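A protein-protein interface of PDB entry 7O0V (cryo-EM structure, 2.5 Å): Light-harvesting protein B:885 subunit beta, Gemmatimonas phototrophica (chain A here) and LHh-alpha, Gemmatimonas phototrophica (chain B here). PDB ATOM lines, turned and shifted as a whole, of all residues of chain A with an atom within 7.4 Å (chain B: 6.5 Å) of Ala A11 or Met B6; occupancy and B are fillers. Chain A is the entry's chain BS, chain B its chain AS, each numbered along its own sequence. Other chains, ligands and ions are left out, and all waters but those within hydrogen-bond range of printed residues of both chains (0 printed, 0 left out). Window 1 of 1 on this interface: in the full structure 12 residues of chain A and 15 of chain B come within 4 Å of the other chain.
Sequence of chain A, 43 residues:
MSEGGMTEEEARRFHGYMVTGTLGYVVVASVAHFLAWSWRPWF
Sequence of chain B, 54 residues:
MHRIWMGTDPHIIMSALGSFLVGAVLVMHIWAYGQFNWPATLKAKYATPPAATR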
ATOM      1  N   GLY A   4      26.342  37.224  14.888  1.00  0.00           N
ATOM      2  CA  GLY A   4      25.276  37.665  15.768  1.00  0.00           C
ATOM      3  C   GLY A   4      23.888  37.334  15.253  1.00  0.00           C
ATOM      4  O   GLY A   4      22.887  37.691  15.873  1.00  0.00           O
ATOM      5  N   GLY A   5      23.829  36.653  14.112  1.00  0.00           N
ATOM      6  CA  GLY A   5      22.574  36.141  13.595  1.00  0.00           C
ATOM      7  C   GLY A   5      22.137  34.833  14.223  1.00  0.00           C
ATOM      8  O   GLY A   5      22.295  34.631  15.430  1.00  0.00           O
ATOM      9  N   MET A   6      21.570  33.945  13.405  1.00  0.00           N
ATOM     10  CA  MET A   6      21.042  32.670  13.878  1.00  0.00           C
ATOM     11  C   MET A   6      22.073  31.867  14.665  1.00  0.00           C
ATOM     12  O   MET A   6      23.210  31.683  14.224  1.00  0.00           O
ATOM     13  CB  MET A   6      20.520  31.846  12.700  1.00  0.00           C
ATOM     14  CG  MET A   6      19.197  32.351  12.149  1.00  0.00           C
ATOM     15  SD  MET A   6      18.506  31.303  10.856  1.00  0.00           S
ATOM     16  CE  MET A   6      19.359  31.929   9.414  1.00  0.00           C
ATOM     17  N   THR A   7      21.660  31.397  15.842  1.00  0.00           N
ATOM     18  CA  THR A   7      22.371  30.370  16.588  1.00  0.00           C
ATOM     19  C   THR A   7      22.108  28.994  15.973  1.00  0.00           C
ATOM     20  O   THR A   7      21.229  28.821  15.125  1.00  0.00           O
ATOM     21  CB  THR A   7      21.954  30.386  18.057  1.00  0.00           C
ATOM     22  OG1 THR A   7      20.545  30.143  18.156  1.00  0.00           O
ATOM     23  CG2 THR A   7      22.268  31.736  18.686  1.00  0.00           C
ATOM     24  N   GLU A   8      22.898  28.006  16.406  1.00  0.00           N
ATOM     25  CA  GLU A   8      22.863  26.686  15.776  1.00  0.00           C
ATOM     26  C   GLU A   8      21.473  26.054  15.800  1.00  0.00           C
ATOM     27  O   GLU A   8      21.080  25.384  14.837  1.00  0.00           O
ATOM     28  CB  GLU A   8      23.877  25.748  16.433  1.00  0.00           C
ATOM     29  CG  GLU A   8      23.990  24.414  15.705  1.00  0.00           C
ATOM     30  CD  GLU A   8      25.363  23.785  15.806  1.00  0.00           C
ATOM     31  OE1 GLU A   8      26.070  24.040  16.802  1.00  0.00           O
ATOM     32  OE2 GLU A   8      25.734  23.029  14.882  1.00  0.00           O
ATOM     33  N   GLU A   9      20.707  26.253  16.873  1.00  0.00           N
ATOM     34  CA  GLU A   9      19.373  25.661  16.891  1.00  0.00           C
ATOM     35  C   GLU A   9      18.384  26.439  16.034  1.00  0.00           C
ATOM     36  O   GLU A   9      17.480  25.838  15.443  1.00  0.00           O
ATOM     37  CB  GLU A   9      18.856  25.546  18.328  1.00  0.00           C
ATOM     38  CG  GLU A   9      17.483  24.875  18.465  1.00  0.00           C
ATOM     39  CD  GLU A   9      17.381  23.513  17.783  1.00  0.00           C
ATOM     40  OE1 GLU A   9      18.419  22.854  17.560  1.00  0.00           O
ATOM     41  OE2 GLU A   9      16.246  23.100  17.464  1.00  0.00           O
ATOM     42  N   GLU A  10      18.536  27.761  15.944  1.00  0.00           N
ATOM     43  CA  GLU A  10      17.792  28.516  14.942  1.00  0.00           C
ATOM     44  C   GLU A  10      18.150  28.055  13.535  1.00  0.00           C
ATOM     45  O   GLU A  10      17.269  27.865  12.689  1.00  0.00           O
ATOM     46  CB  GLU A  10      18.066  30.011  15.101  1.00  0.00           C
ATOM     47  CG  GLU A  10      17.497  30.625  16.367  1.00  0.00           C
ATOM     48  CD  GLU A  10      18.056  32.007  16.641  1.00  0.00           C
ATOM     49  OE1 GLU A  10      19.266  32.111  16.931  1.00  0.00           O
ATOM     50  OE2 GLU A  10      17.288  32.990  16.567  1.00  0.00           O
ATOM     51  N   ALA A  11      19.447  27.869  13.272  1.00  0.00           N
ATOM     52  CA  ALA A  11      19.899  27.401  11.965  1.00  0.00           C
ATOM     53  C   ALA A  11      19.399  25.994  11.649  1.00  0.00           C
ATOM     54  O   ALA A  11      19.005  25.714  10.511  1.00  0.00           O
ATOM     55  CB  ALA A  11      21.424  27.452  11.898  1.00  0.00           C
ATOM     56  N   ARG A  12      19.414  25.092  12.634  1.00  0.00           N
ATOM     57  CA  ARG A  12      18.857  23.758  12.417  1.00  0.00           C
ATOM     58  C   ARG A  12      17.372  23.813  12.069  1.00  0.00           C
ATOM     59  O   ARG A  12      16.910  23.091  11.180  1.00  0.00           O
ATOM     60  CB  ARG A  12      19.101  22.878  13.644  1.00  0.00           C
ATOM     61  CG  ARG A  12      18.658  21.436  13.451  1.00  0.00           C
ATOM     62  CD  ARG A  12      18.992  20.556  14.649  1.00  0.00           C
ATOM     63  NE  ARG A  12      20.428  20.339  14.785  1.00  0.00           N
ATOM     64  CZ  ARG A  12      21.199  20.912  15.698  1.00  0.00           C
ATOM     65  NH1 ARG A  12      20.706  21.757  16.589  1.00  0.00           N
ATOM     66  NH2 ARG A  12      22.499  20.631  15.717  1.00  0.00           N
ATOM     67  N   ARG A  13      16.612  24.660  12.762  1.00  0.00           N
ATOM     68  CA  ARG A  13      15.217  24.894  12.404  1.00  0.00           C
ATOM     69  C   ARG A  13      15.100  25.483  11.001  1.00  0.00           C
ATOM     70  O   ARG A  13      14.396  24.946  10.139  1.00  0.00           O
ATOM     71  CB  ARG A  13      14.569  25.810  13.444  1.00  0.00           C
ATOM     72  CG  ARG A  13      13.923  25.060  14.596  1.00  0.00           C
ATOM     73  CD  ARG A  13      13.917  25.872  15.882  1.00  0.00           C
ATOM     74  NE  ARG A  13      13.604  27.279  15.672  1.00  0.00           N
ATOM     75  CZ  ARG A  13      13.737  28.219  16.599  1.00  0.00           C
ATOM     76  NH1 ARG A  13      13.954  27.912  17.866  1.00  0.00           N
ATOM     77  NH2 ARG A  13      13.584  29.494  16.256  1.00  0.00           N
ATOM     78  N   PHE A  14      15.785  26.604  10.768  1.00  0.00           N
ATOM     79  CA  PHE A  14      15.730  27.302   9.485  1.00  0.00           C
ATOM     80  C   PHE A  14      16.093  26.395   8.311  1.00  0.00           C
ATOM     81  O   PHE A  14      15.432  26.430   7.267  1.00  0.00           O
ATOM     82  CB  PHE A  14      16.665  28.513   9.546  1.00  0.00           C
ATOM     83  CG  PHE A  14      16.669  29.358   8.306  1.00  0.00           C
ATOM     84  CD1 PHE A  14      15.770  30.399   8.159  1.00  0.00           C
ATOM     85  CD2 PHE A  14      17.603  29.141   7.307  1.00  0.00           C
ATOM     86  CE1 PHE A  14      15.783  31.187   7.025  1.00  0.00           C
ATOM     87  CE2 PHE A  14      17.622  29.928   6.176  1.00  0.00           C
ATOM     88  CZ  PHE A  14      16.709  30.951   6.033  1.00  0.00           C
ATOM     89  N   HIS A  15      17.140  25.581   8.460  1.00  0.00           N
ATOM     90  CA  HIS A  15      17.524  24.642   7.406  1.00  0.00           C
ATOM     91  C   HIS A  15      16.397  23.691   7.015  1.00  0.00           C
ATOM     92  O   HIS A  15      16.152  23.468   5.824  1.00  0.00           O
ATOM     93  CB  HIS A  15      18.745  23.837   7.840  1.00  0.00           C
ATOM     94  CG  HIS A  15      19.305  22.974   6.756  1.00  0.00           C
ATOM     95  ND1 HIS A  15      19.935  23.483   5.642  1.00  0.00           N
ATOM     96  CD2 HIS A  15      19.304  21.628   6.605  1.00  0.00           C
ATOM     97  CE1 HIS A  15      20.310  22.489   4.857  1.00  0.00           C
ATOM     98  NE2 HIS A  15      19.939  21.353   5.419  1.00  0.00           N
ATOM     99  N   GLY A  16      15.706  23.112   7.997  1.00  0.00           N
ATOM    100  CA  GLY A  16      14.640  22.176   7.673  1.00  0.00           C
ATOM    101  C   GLY A  16      13.519  22.795   6.859  1.00  0.00           C
ATOM    102  O   GLY A  16      13.000  22.175   5.928  1.00  0.00           O
ATOM    103  N   TYR A  17      13.135  24.023   7.195  1.00  0.00           N
ATOM    104  CA  TYR A  17      12.128  24.730   6.413  1.00  0.00           C
ATOM    105  C   TYR A  17      12.630  25.102   5.024  1.00  0.00           C
ATOM    106  O   TYR A  17      11.901  24.955   4.036  1.00  0.00           O
ATOM    107  CB  TYR A  17      11.656  25.962   7.179  1.00  0.00           C
ATOM    108  CG  TYR A  17      10.763  25.590   8.333  1.00  0.00           C
ATOM    109  CD1 TYR A  17       9.503  25.059   8.104  1.00  0.00           C
ATOM    110  CD2 TYR A  17      11.191  25.722   9.646  1.00  0.00           C
ATOM    111  CE1 TYR A  17       8.679  24.699   9.147  1.00  0.00           C
ATOM    112  CE2 TYR A  17      10.375  25.360  10.700  1.00  0.00           C
ATOM    113  CZ  TYR A  17       9.119  24.849  10.442  1.00  0.00           C
ATOM    114  OH  TYR A  17       8.298  24.481  11.483  1.00  0.00           O
ATOM    115  N   HIS B   2      23.172  22.303   8.166  1.00  0.00           N
ATOM    116  CA  HIS B   2      22.374  23.435   8.630  1.00  0.00           C
ATOM    117  C   HIS B   2      23.168  24.653   9.092  1.00  0.00           C
ATOM    118  O   HIS B   2      22.686  25.779   9.009  1.00  0.00           O
ATOM    119  CB  HIS B   2      21.516  22.982   9.804  1.00  0.00           C
ATOM    120  CG  HIS B   2      22.323  22.547  10.986  1.00  0.00           C
ATOM    121  ND1 HIS B   2      22.999  21.346  11.026  1.00  0.00           N
ATOM    122  CD2 HIS B   2      22.609  23.177  12.150  1.00  0.00           C
ATOM    123  CE1 HIS B   2      23.642  21.244  12.174  1.00  0.00           C
ATOM    124  NE2 HIS B   2      23.424  22.343  12.874  1.00  0.00           N
ATOM    125  N   ARG B   3      24.376  24.435   9.598  1.00  0.00           N
ATOM    126  CA  ARG B   3      25.080  25.508  10.290  1.00  0.00           C
ATOM    127  C   ARG B   3      25.730  26.516   9.345  1.00  0.00           C
ATOM    128  O   ARG B   3      26.340  27.480   9.820  1.00  0.00           O
ATOM    129  CB  ARG B   3      26.057  24.927  11.323  1.00  0.00           C
ATOM    130  CG  ARG B   3      27.449  24.584  10.893  1.00  0.00           C
ATOM    131  CD  ARG B   3      28.246  24.198  12.141  1.00  0.00           C
ATOM    132  NE  ARG B   3      27.658  23.081  12.875  1.00  0.00           N
ATOM    133  CZ  ARG B   3      27.682  21.810  12.497  1.00  0.00           C
ATOM    134  NH1 ARG B   3      28.302  21.426  11.394  1.00  0.00           N
ATOM    135  NH2 ARG B   3      27.078  20.899  13.253  1.00  0.00           N
ATOM    136  N   ILE B   4      25.611  26.321   8.030  1.00  0.00           N
ATOM    137  CA  ILE B   4      25.912  27.391   7.080  1.00  0.00           C
ATOM    138  C   ILE B   4      25.028  28.612   7.320  1.00  0.00           C
ATOM    139  O   ILE B   4      25.430  29.743   7.020  1.00  0.00           O
ATOM    140  CB  ILE B   4      25.779  26.871   5.631  1.00  0.00           C
ATOM    141  CG1 ILE B   4      26.388  27.866   4.638  1.00  0.00           C
ATOM    142  CG2 ILE B   4      24.325  26.576   5.286  1.00  0.00           C
ATOM    143  CD1 ILE B   4      27.847  28.171   4.878  1.00  0.00           C
ATOM    144  N   TRP B   5      23.827  28.418   7.864  1.00  0.00           N
ATOM    145  CA  TRP B   5      22.937  29.535   8.160  1.00  0.00           C
ATOM    146  C   TRP B   5      23.319  30.313   9.412  1.00  0.00           C
ATOM    147  O   TRP B   5      22.773  31.401   9.625  1.00  0.00           O
ATOM    148  CB  TRP B   5      21.492  29.041   8.275  1.00  0.00           C
ATOM    149  CG  TRP B   5      21.096  28.186   7.121  1.00  0.00           C
ATOM    150  CD1 TRP B   5      20.749  26.869   7.156  1.00  0.00           C
ATOM    151  CD2 TRP B   5      21.061  28.574   5.745  1.00  0.00           C
ATOM    152  NE1 TRP B   5      20.475  26.418   5.890  1.00  0.00           N
ATOM    153  CE2 TRP B   5      20.661  27.446   5.005  1.00  0.00           C
ATOM    154  CE3 TRP B   5      21.316  29.770   5.069  1.00  0.00           C
ATOM    155  CZ2 TRP B   5      20.512  27.478   3.626  1.00  0.00           C
ATOM    156  CZ3 TRP B   5      21.168  29.798   3.701  1.00  0.00           C
ATOM    157  CH2 TRP B   5      20.773  28.660   2.995  1.00  0.00           C
ATOM    158  N   MET B   6      24.215  29.790  10.247  1.00  0.00           N
ATOM    159  CA  MET B   6      24.581  30.485  11.474  1.00  0.00           C
ATOM    160  C   MET B   6      25.174  31.856  11.166  1.00  0.00           C
ATOM    161  O   MET B   6      25.852  32.054  10.154  1.00  0.00           O
ATOM    162  CB  MET B   6      25.581  29.658  12.284  1.00  0.00           C
ATOM    163  CG  MET B   6      25.043  28.323  12.767  1.00  0.00           C
ATOM    164  SD  MET B   6      26.083  27.581  14.038  1.00  0.00           S
ATOM    165  CE  MET B   6      27.701  27.727  13.286  1.00  0.00           C
ATOM    166  N   GLY B   7      24.910  32.811  12.059  1.00  0.00           N
ATOM    167  CA  GLY B   7      25.376  34.174  11.910  1.00  0.00           C
ATOM    168  C   GLY B   7      24.665  35.010  10.868  1.00  0.00           C
ATOM    169  O   GLY B   7      24.884  36.227  10.828  1.00  0.00           O
ATOM    170  N   THR B   8      23.825  34.414  10.028  1.00  0.00           N
ATOM    171  CA  THR B   8      23.065  35.148   9.025  1.00  0.00           C
ATOM    172  C   THR B   8      21.700  35.561   9.573  1.00  0.00           C
ATOM    173  O   THR B   8      21.205  35.012  10.560  1.00  0.00           O
ATOM    174  CB  THR B   8      22.892  34.316   7.753  1.00  0.00           C
ATOM    175  OG1 THR B   8      21.903  33.303   7.972  1.00  0.00           O
ATOM    176  CG2 THR B   8      24.207  33.662   7.359  1.00  0.00           C
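The backbone carbonyl oxygen (O) of Trp B5 lies within hydrogen-bond range of the side-chain hydroxyl (OG1) of Thr B8. The side-chain carboxylate of Glu A9 is in salt-bridge range of the guanidinium group of Arg A12 (2.7 Å).
Of chain B, only His B2 (3.6 Å), Trp B5 (3.95 Å) and Met B6 (3.8 Å) come within 4 Å of Ala A11. Printed residues of chain A within 4 Å of Met B6: Met A6, Glu A8 and Ala A11. Printed residues of chain A within 4 Å of Arg B3: Glu A8. Of the printed residues of chain A, Gly B7 touches Gly A5 (3.5 Å) and Met A6 (3.0 Å). Of the printed residues of chain B, His A15 touches His B2 and Trp B5. The nearest residue of chain A that does not touch Met B6 is Thr A7 (4.4 Å).
Hydrophobic or aromatic side chains of chain A within 4 Å of the printed part of chain B: Met A6, Ala A11, Phe A14 and His A15. Of the 7 printed residues of chain B, 6 touch a printed residue of chain A. Hydrophobic or aromatic side chains of chain B within 4 Å of the printed part of chain A: His B2, Trp B5 and Met B6. Among the printed residues, 16 pairs touch across the chains. Among the printed residues, Asp or Glu carboxylates within 4 Å of a Lys or Arg side-chain nitrogen of the other chain: Glu A8 with Arg B3 (2.8 Å).
NE2 of His B2 sits at hydrogen-bond distance from OE2 of Glu A8 (3.1 Å). NH2 of Arg A12 is in hydrogen-bond range of NE2 of His B2 (3.4 Å). The guanidinium group (NE) of Arg B3 lies within salt-bridge range of the side-chain carboxylate (OE2) of Glu A8. NE1 of Trp B5 sits at hydrogen-bond distance from ND1 of His A15 (3.0 Å). The backbone NH (N) of Gly A5 lies within hydrogen-bond range of the backbone carbonyl oxygen (O) of Gly B7 (3.5 Å). N of Gly B7 sits at hydrogen-bond distance from O of Met A6, 3.0 Å away. The backbone carbonyl oxygen of Thr B8 sits at hydrogen-bond distance from the backbone NH of Met A6 (3.1 Å).
Thr B8 touches Gly A5 (O to CA, 3.5 Å). Met A6 touches Trp B5. Met B6 touches Met A6. Met B6 touches Glu A8 (SD to CB, 3.7 Å). Ala A11 touches His B2 (CB to O, 3.6 Å). Trp B5 touches Ala A11. CB of Ala A11 touches CG of Met B6 (3.8 Å). Phe A14 touches Trp B5 (CD2 to CG, 3.6 Å). CB of His A15 touches CB of His B2, 3.5 Å away.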
